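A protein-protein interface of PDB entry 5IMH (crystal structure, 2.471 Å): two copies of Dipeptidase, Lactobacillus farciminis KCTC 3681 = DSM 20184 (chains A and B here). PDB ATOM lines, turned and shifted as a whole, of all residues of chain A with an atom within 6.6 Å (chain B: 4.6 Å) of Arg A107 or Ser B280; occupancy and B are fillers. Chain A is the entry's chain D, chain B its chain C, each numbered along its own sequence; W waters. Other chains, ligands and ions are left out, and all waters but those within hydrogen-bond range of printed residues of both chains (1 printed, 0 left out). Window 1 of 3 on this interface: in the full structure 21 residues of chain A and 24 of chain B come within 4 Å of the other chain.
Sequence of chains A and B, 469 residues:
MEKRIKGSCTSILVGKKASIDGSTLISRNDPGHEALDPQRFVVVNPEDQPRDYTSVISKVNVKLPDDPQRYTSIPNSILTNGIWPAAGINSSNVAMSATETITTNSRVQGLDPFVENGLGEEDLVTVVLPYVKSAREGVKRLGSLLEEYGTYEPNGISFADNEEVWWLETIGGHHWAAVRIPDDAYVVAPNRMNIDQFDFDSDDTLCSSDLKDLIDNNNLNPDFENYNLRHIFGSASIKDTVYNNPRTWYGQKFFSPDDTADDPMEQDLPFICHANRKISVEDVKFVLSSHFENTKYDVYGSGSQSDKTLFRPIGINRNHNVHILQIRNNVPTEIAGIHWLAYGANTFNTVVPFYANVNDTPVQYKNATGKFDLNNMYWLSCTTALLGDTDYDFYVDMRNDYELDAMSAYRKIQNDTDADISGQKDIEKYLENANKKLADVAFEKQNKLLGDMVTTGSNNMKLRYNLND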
ATOM      1  N   ASN A 105      27.777   3.468   4.736  1.00  0.00           N
ATOM      2  CA  ASN A 105      26.374   3.102   4.939  1.00  0.00           C
ATOM      3  C   ASN A 105      26.240   1.994   5.987  1.00  0.00           C
ATOM      4  O   ASN A 105      27.226   1.371   6.357  1.00  0.00           O
ATOM      5  CB  ASN A 105      25.714   2.692   3.617  1.00  0.00           C
ATOM      6  CG  ASN A 105      26.259   1.386   3.057  1.00  0.00           C
ATOM      7  OD1 ASN A 105      26.098   0.312   3.656  1.00  0.00           O
ATOM      8  ND2 ASN A 105      26.882   1.468   1.886  1.00  0.00           N
ATOM      9  N   SER A 106      25.021   1.738   6.445  1.00  0.00           N
ATOM     10  CA  SER A 106      24.825   0.843   7.584  1.00  0.00           C
ATOM     11  C   SER A 106      24.973  -0.639   7.245  1.00  0.00           C
ATOM     12  O   SER A 106      25.147  -1.468   8.151  1.00  0.00           O
ATOM     13  CB  SER A 106      23.450   1.088   8.225  1.00  0.00           C
ATOM     14  OG  SER A 106      22.420   1.150   7.254  1.00  0.00           O
ATOM     15  N   ARG A 107      24.914  -0.980   5.959  1.00  0.00           N
ATOM     16  CA  ARG A 107      25.040  -2.376   5.554  1.00  0.00           C
ATOM     17  C   ARG A 107      26.483  -2.872   5.743  1.00  0.00           C
ATOM     18  O   ARG A 107      26.712  -3.951   6.320  1.00  0.00           O
ATOM     19  CB  ARG A 107      24.565  -2.554   4.106  1.00  0.00           C
ATOM     20  CG  ARG A 107      23.043  -2.531   3.958  1.00  0.00           C
ATOM     21  CD  ARG A 107      22.565  -2.397   2.476  1.00  0.00           C
ATOM     22  NE  ARG A 107      23.210  -1.293   1.758  1.00  0.00           N
ATOM     23  CZ  ARG A 107      22.819  -0.022   1.839  1.00  0.00           C
ATOM     24  NH1 ARG A 107      21.787   0.310   2.605  1.00  0.00           N
ATOM     25  NH2 ARG A 107      23.468   0.921   1.175  1.00  0.00           N
ATOM     26  N   VAL A 108      27.454  -2.084   5.287  1.00  0.00           N
ATOM     27  CA  VAL A 108      28.857  -2.418   5.523  1.00  0.00           C
ATOM     28  C   VAL A 108      29.254  -2.158   6.979  1.00  0.00           C
ATOM     29  O   VAL A 108      30.008  -2.941   7.564  1.00  0.00           O
ATOM     30  CB  VAL A 108      29.807  -1.649   4.594  1.00  0.00           C
ATOM     31  CG1 VAL A 108      29.559  -0.158   4.655  1.00  0.00           C
ATOM     32  CG2 VAL A 108      31.254  -1.975   4.945  1.00  0.00           C
ATOM     33  N   GLN A 109      28.723  -1.101   7.589  1.00  0.00           N
ATOM     34  CA  GLN A 109      29.052  -0.841   8.981  1.00  0.00           C
ATOM     35  C   GLN A 109      28.536  -1.993   9.838  1.00  0.00           C
ATOM     36  O   GLN A 109      29.149  -2.338  10.844  1.00  0.00           O
ATOM     37  CB  GLN A 109      28.469   0.498   9.462  1.00  0.00           C
ATOM     38  CG  GLN A 109      29.175   1.743   8.918  1.00  0.00           C
ATOM     39  CD  GLN A 109      30.588   1.901   9.474  1.00  0.00           C
ATOM     40  OE1 GLN A 109      30.852   1.597  10.651  1.00  0.00           O
ATOM     41  NE2 GLN A 109      31.512   2.366   8.621  1.00  0.00           N
ATOM     42  N   GLY A 110      27.446  -2.623   9.405  1.00  0.00           N
ATOM     43  CA  GLY A 110      26.893  -3.772  10.106  1.00  0.00           C
ATOM     44  C   GLY A 110      27.776  -5.016  10.061  1.00  0.00           C
ATOM     45  O   GLY A 110      27.556  -5.960  10.824  1.00  0.00           O
ATOM     46  N   LEU A 111      28.766  -5.030   9.165  1.00  0.00           N
ATOM     47  CA  LEU A 111      29.685  -6.171   9.047  1.00  0.00           C
ATOM     48  C   LEU A 111      31.084  -5.899   9.594  1.00  0.00           C
ATOM     49  O   LEU A 111      31.678  -6.747  10.256  1.00  0.00           O
ATOM     50  CB  LEU A 111      29.802  -6.617   7.587  1.00  0.00           C
ATOM     51  CG  LEU A 111      28.598  -7.310   6.966  1.00  0.00           C
ATOM     52  CD1 LEU A 111      28.890  -7.475   5.489  1.00  0.00           C
ATOM     53  CD2 LEU A 111      28.329  -8.661   7.635  1.00  0.00           C
ATOM     54  N   ASP A 112      31.614  -4.728   9.266  1.00  0.00           N
ATOM     55  CA  ASP A 112      32.936  -4.300   9.705  1.00  0.00           C
ATOM     56  C   ASP A 112      32.810  -2.891  10.316  1.00  0.00           C
ATOM     57  O   ASP A 112      33.135  -1.889   9.671  1.00  0.00           O
ATOM     58  CB  ASP A 112      33.927  -4.288   8.542  1.00  0.00           C
ATOM     59  CG  ASP A 112      35.327  -3.828   8.962  1.00  0.00           C
ATOM     60  OD1 ASP A 112      35.610  -3.794  10.183  1.00  0.00           O
ATOM     61  OD2 ASP A 112      36.143  -3.478   8.077  1.00  0.00           O
ATOM     62  N   ASN A 218      27.919 -11.310   1.152  1.00  0.00           N
ATOM     63  CA  ASN A 218      27.040 -10.663   2.128  1.00  0.00           C
ATOM     64  C   ASN A 218      25.911  -9.776   1.571  1.00  0.00           C
ATOM     65  O   ASN A 218      25.349  -8.949   2.300  1.00  0.00           O
ATOM     66  CB  ASN A 218      27.900  -9.839   3.080  1.00  0.00           C
ATOM     67  CG  ASN A 218      28.734 -10.704   3.995  1.00  0.00           C
ATOM     68  OD1 ASN A 218      28.209 -11.292   4.929  1.00  0.00           O
ATOM     69  ND2 ASN A 218      30.036 -10.775   3.744  1.00  0.00           N
ATOM     70  N   ASN A 219      25.567  -9.958   0.299  1.00  0.00           N
ATOM     71  CA  ASN A 219      24.503  -9.169  -0.357  1.00  0.00           C
ATOM     72  C   ASN A 219      24.724  -7.675  -0.218  1.00  0.00           C
ATOM     73  O   ASN A 219      23.799  -6.951   0.166  1.00  0.00           O
ATOM     74  CB  ASN A 219      23.120  -9.487   0.213  1.00  0.00           C
ATOM     75  CG  ASN A 219      22.738 -10.925   0.038  1.00  0.00           C
ATOM     76  OD1 ASN A 219      22.549 -11.393  -1.079  1.00  0.00           O
ATOM     77  ND2 ASN A 219      22.566 -11.629   1.150  1.00  0.00           N
ATOM     78  N   LEU A 220      25.960  -7.229  -0.432  1.00  0.00           N
ATOM     79  CA  LEU A 220      26.281  -5.814  -0.332  1.00  0.00           C
ATOM     80  C   LEU A 220      26.076  -5.085  -1.645  1.00  0.00           C
ATOM     81  O   LEU A 220      25.958  -3.857  -1.666  1.00  0.00           O
ATOM     82  CB  LEU A 220      27.724  -5.617   0.121  1.00  0.00           C
ATOM     83  CG  LEU A 220      27.989  -5.882   1.598  1.00  0.00           C
ATOM     84  CD1 LEU A 220      29.423  -5.510   1.959  1.00  0.00           C
ATOM     85  CD2 LEU A 220      26.979  -5.138   2.443  1.00  0.00           C
ATOM     86  N   PRO A 222      24.254  -3.723  -4.733  1.00  0.00           N
ATOM     87  CA  PRO A 222      22.913  -3.341  -5.173  1.00  0.00           C
ATOM     88  C   PRO A 222      22.755  -3.394  -6.722  1.00  0.00           C
ATOM     89  O   PRO A 222      21.633  -3.373  -7.242  1.00  0.00           O
ATOM     90  CB  PRO A 222      22.792  -1.905  -4.655  1.00  0.00           C
ATOM     91  CG  PRO A 222      24.171  -1.370  -4.773  1.00  0.00           C
ATOM     92  CD  PRO A 222      25.094  -2.543  -4.468  1.00  0.00           C
ATOM     93  N   HIS A 231      28.468   2.890  -4.707  1.00  0.00           N
ATOM     94  CA  HIS A 231      27.141   2.288  -4.663  1.00  0.00           C
ATOM     95  C   HIS A 231      27.065   1.252  -3.564  1.00  0.00           C
ATOM     96  O   HIS A 231      26.068   1.156  -2.849  1.00  0.00           O
ATOM     97  CB  HIS A 231      26.792   1.622  -5.989  1.00  0.00           C
ATOM     98  CG  HIS A 231      26.420   2.576  -7.074  1.00  0.00           C
ATOM     99  ND1 HIS A 231      26.002   2.153  -8.319  1.00  0.00           N
ATOM    100  CD2 HIS A 231      26.389   3.929  -7.102  1.00  0.00           C
ATOM    101  CE1 HIS A 231      25.745   3.207  -9.071  1.00  0.00           C
ATOM    102  NE2 HIS A 231      25.965   4.297  -8.353  1.00  0.00           N
ATOM    103  N   ILE A 232      28.131   0.461  -3.460  1.00  0.00           N
ATOM    104  CA  ILE A 232      28.192  -0.683  -2.561  1.00  0.00           C
ATOM    105  C   ILE A 232      28.441  -0.253  -1.126  1.00  0.00           C
ATOM    106  O   ILE A 232      27.712  -0.665  -0.229  1.00  0.00           O
ATOM    107  CB  ILE A 232      29.313  -1.669  -3.007  1.00  0.00           C
ATOM    108  CG1 ILE A 232      29.030  -2.239  -4.390  1.00  0.00           C
ATOM    109  CG2 ILE A 232      29.481  -2.816  -2.031  1.00  0.00           C
ATOM    110  CD1 ILE A 232      30.235  -2.872  -5.026  1.00  0.00           C
ATOM    111  N   PHE A 233      29.456   0.598  -0.927  1.00  0.00           N
ATOM    112  CA  PHE A 233      29.994   0.961   0.397  1.00  0.00           C
ATOM    113  C   PHE A 233      29.725   2.391   0.820  1.00  0.00           C
ATOM    114  O   PHE A 233      30.041   2.776   1.947  1.00  0.00           O
ATOM    115  CB  PHE A 233      31.512   0.793   0.429  1.00  0.00           C
ATOM    116  CG  PHE A 233      31.981  -0.615   0.251  1.00  0.00           C
ATOM    117  CD1 PHE A 233      31.604  -1.610   1.141  1.00  0.00           C
ATOM    118  CD2 PHE A 233      32.823  -0.939  -0.800  1.00  0.00           C
ATOM    119  CE1 PHE A 233      32.042  -2.903   0.965  1.00  0.00           C
ATOM    120  CE2 PHE A 233      33.263  -2.212  -0.969  1.00  0.00           C
ATOM    121  CZ  PHE A 233      32.873  -3.201  -0.088  1.00  0.00           C
ATOM    122  N   GLY A 234      29.230   3.204  -0.109  1.00  0.00           N
ATOM    123  CA  GLY A 234      29.161   4.639   0.099  1.00  0.00           C
ATOM    124  C   GLY A 234      27.752   5.123   0.334  1.00  0.00           C
ATOM    125  O   GLY A 234      26.904   4.397   0.860  1.00  0.00           O
ATOM    126  N   ILE B  20      17.930  -6.378  -2.247  1.00  0.00           N
ATOM    127  CA  ILE B  20      19.380  -6.497  -2.289  1.00  0.00           C
ATOM    128  C   ILE B  20      19.835  -7.806  -1.625  1.00  0.00           C
ATOM    129  O   ILE B  20      20.901  -8.340  -1.951  1.00  0.00           O
ATOM    130  CB  ILE B  20      20.057  -5.279  -1.602  1.00  0.00           C
ATOM    131  CG1 ILE B  20      21.541  -5.202  -1.958  1.00  0.00           C
ATOM    132  CG2 ILE B  20      19.862  -5.337  -0.099  1.00  0.00           C
ATOM    133  CD1 ILE B  20      22.224  -3.940  -1.464  1.00  0.00           C
ATOM    134  N   LYS B 278      18.920  -3.110  -7.043  1.00  0.00           N
ATOM    135  CA  LYS B 278      18.236  -3.867  -6.011  1.00  0.00           C
ATOM    136  C   LYS B 278      17.935  -2.959  -4.825  1.00  0.00           C
ATOM    137  O   LYS B 278      18.686  -2.016  -4.536  1.00  0.00           O
ATOM    138  CB  LYS B 278      19.076  -5.052  -5.568  1.00  0.00           C
ATOM    139  CG  LYS B 278      19.483  -6.016  -6.695  1.00  0.00           C
ATOM    140  CD  LYS B 278      20.377  -7.095  -6.096  1.00  0.00           C
ATOM    141  CE  LYS B 278      20.828  -8.122  -7.085  1.00  0.00           C
ATOM    142  NZ  LYS B 278      21.640  -9.116  -6.316  1.00  0.00           N
ATOM    143  N   ILE B 279      16.847  -3.268  -4.128  1.00  0.00           N
ATOM    144  CA  ILE B 279      16.312  -2.405  -3.093  1.00  0.00           C
ATOM    145  C   ILE B 279      16.662  -2.870  -1.691  1.00  0.00           C
ATOM    146  O   ILE B 279      16.505  -4.046  -1.372  1.00  0.00           O
ATOM    147  CB  ILE B 279      14.787  -2.323  -3.218  1.00  0.00           C
ATOM    148  CG1 ILE B 279      14.413  -1.853  -4.637  1.00  0.00           C
ATOM    149  CG2 ILE B 279      14.210  -1.459  -2.117  1.00  0.00           C
ATOM    150  CD1 ILE B 279      12.906  -1.813  -4.923  1.00  0.00           C
ATOM    151  N   SER B 280      17.112  -1.939  -0.854  1.00  0.00           N
ATOM    152  CA  SER B 280      17.494  -2.258   0.517  1.00  0.00           C
ATOM    153  C   SER B 280      16.388  -1.900   1.496  1.00  0.00           C
ATOM    154  O   SER B 280      15.455  -1.163   1.156  1.00  0.00           O
ATOM    155  CB  SER B 280      18.777  -1.516   0.904  1.00  0.00           C
ATOM    156  OG  SER B 280      18.531  -0.113   0.975  1.00  0.00           O
ATOM    157  N   VAL B 281      16.511  -2.400   2.721  1.00  0.00           N
ATOM    158  CA  VAL B 281      15.592  -1.990   3.767  1.00  0.00           C
ATOM    159  C   VAL B 281      15.736  -0.475   3.957  1.00  0.00           C
ATOM    160  O   VAL B 281      14.726   0.232   4.120  1.00  0.00           O
ATOM    161  CB  VAL B 281      15.841  -2.747   5.060  1.00  0.00           C
ATOM    162  CG1 VAL B 281      15.084  -2.114   6.219  1.00  0.00           C
ATOM    163  CG2 VAL B 281      15.429  -4.196   4.876  1.00  0.00           C
ATOM    164  N   GLU B 282      16.979   0.017   3.892  1.00  0.00           N
ATOM    165  CA  GLU B 282      17.243   1.450   3.990  1.00  0.00           C
ATOM    166  C   GLU B 282      16.546   2.274   2.888  1.00  0.00           C
ATOM    167  O   GLU B 282      16.061   3.371   3.156  1.00  0.00           O
ATOM    168  CB  GLU B 282      18.749   1.734   3.975  1.00  0.00           C
ATOM    169  CG  GLU B 282      19.470   1.359   5.290  1.00  0.00           C
ATOM    170  CD  GLU B 282      19.906  -0.122   5.389  1.00  0.00           C
ATOM    171  OE1 GLU B 282      19.644  -0.915   4.443  1.00  0.00           O
ATOM    172  OE2 GLU B 282      20.497  -0.494   6.438  1.00  0.00           O
ATOM    173  N   ASP B 283      16.483   1.753   1.665  1.00  0.00           N
ATOM    174  CA  ASP B 283      15.826   2.469   0.570  1.00  0.00           C
ATOM    175  C   ASP B 283      14.331   2.625   0.896  1.00  0.00           C
ATOM    176  O   ASP B 283      13.761   3.714   0.781  1.00  0.00           O
ATOM    177  CB  ASP B 283      15.990   1.738  -0.777  1.00  0.00           C
ATOM    178  CG  ASP B 283      17.437   1.663  -1.271  1.00  0.00           C
ATOM    179  OD1 ASP B 283      18.243   2.598  -1.088  1.00  0.00           O
ATOM    180  OD2 ASP B 283      17.776   0.617  -1.866  1.00  0.00           O
ATOM    181  N   VAL B 284      13.702   1.520   1.289  1.00  0.00           N
ATOM    182  CA  VAL B 284      12.278   1.530   1.591  1.00  0.00           C
ATOM    183  C   VAL B 284      11.972   2.479   2.756  1.00  0.00           C
ATOM    184  O   VAL B 284      11.056   3.318   2.678  1.00  0.00           O
ATOM    185  CB  VAL B 284      11.765   0.110   1.920  1.00  0.00           C
ATOM    186  CG1 VAL B 284      10.357   0.171   2.443  1.00  0.00           C
ATOM    187  CG2 VAL B 284      11.838  -0.783   0.689  1.00  0.00           C
ATOM    188  N   ARG B 411      22.099  -3.867  12.762  1.00  0.00           N
ATOM    189  CA  ARG B 411      22.548  -4.846  11.783  1.00  0.00           C
ATOM    190  C   ARG B 411      23.679  -5.719  12.306  1.00  0.00           C
ATOM    191  O   ARG B 411      23.771  -6.890  11.954  1.00  0.00           O
ATOM    192  CB  ARG B 411      22.990  -4.142  10.505  1.00  0.00           C
ATOM    193  CG  ARG B 411      21.827  -3.671   9.636  1.00  0.00           C
ATOM    194  CD  ARG B 411      22.223  -3.601   8.179  1.00  0.00           C
ATOM    195  NE  ARG B 411      21.127  -3.234   7.287  1.00  0.00           N
ATOM    196  CZ  ARG B 411      20.348  -4.125   6.669  1.00  0.00           C
ATOM    197  NH1 ARG B 411      20.526  -5.420   6.885  1.00  0.00           N
ATOM    198  NH2 ARG B 411      19.381  -3.727   5.849  1.00  0.00           N
HETATM  199  O   HOH W   1      20.148   1.387  -0.004  1.00  0.00           O
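Among the printed residues, pairs that only touch across the chains: Asn A219 with Ile B20, Ser A106 with Arg B411, Arg A107 with Ser B280, Leu A220 with Ile B20, Pro A222 with Ile B20, Arg A107 with Arg B411 and Gly A110 with Arg B411.
Of the 9 printed residues of chain B, 5 touch a printed residue of chain A.
Among the printed residues, Asp or Glu carboxylates within 4 Å of a Lys or Arg side-chain nitrogen of the other chain: Arg A107 with Glu B282.
N of Ile B20 is in hydrogen-bond range of O of Ile B279 (2.9 Å).
The side-chain hydroxyl (OG) of Ser B280 sits close to the backbone NH (N) of Glu B282 (3.3 Å).
The backbone NH of Ser B280 is in hydrogen-bond range of the side-chain carboxylate of Asp B283 (2.8 Å).
NE of Arg B411 lies within salt-bridge range of OE2 of Glu B282, at 2.9 Å.
The side-chain amide oxygen of Asn A105 lies within hydrogen-bond range of the backbone NH of Arg A107 (2.9 Å).
No position is printed for both chains.
Of chain B, only Ser B280 (3.7 Å), Glu B282 (3.1 Å) and Arg B411 (3.9 Å) come within 4 Å of Arg A107.
Of the printed residues of chain B, Asn A219 touches Ile B20 (3.3 Å).
Ser B280 touches just one residue of chain A: Arg A107 (3.7 Å).
Printed residues of chain A within 4 Å of Glu B282: Ser A106 and Arg A107.
The nearest printed residue of chain A that does not touch Glu B282 is Asn A105 (6.3 Å).
Water W1 lies within hydrogen-bond range of the side-chain hydroxyl (OG) of Ser B280 (2.4 Å), the side-chain carboxylate (OD1) of Asp B283 (2.5 Å) and the guanidinium group (NH1) of Arg A107 (3.3 Å).
N of Lys B278 sits at hydrogen-bond distance from O of Pro A222, at 2.7 Å.
The side-chain carboxylate of Glu B282 lies within hydrogen-bond range of the side-chain hydroxyl of Ser A106.
The side-chain carboxylate (OE1) of Glu B282 is in salt-bridge range of the guanidinium group (NH1) of Arg A107 (3.1 Å).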
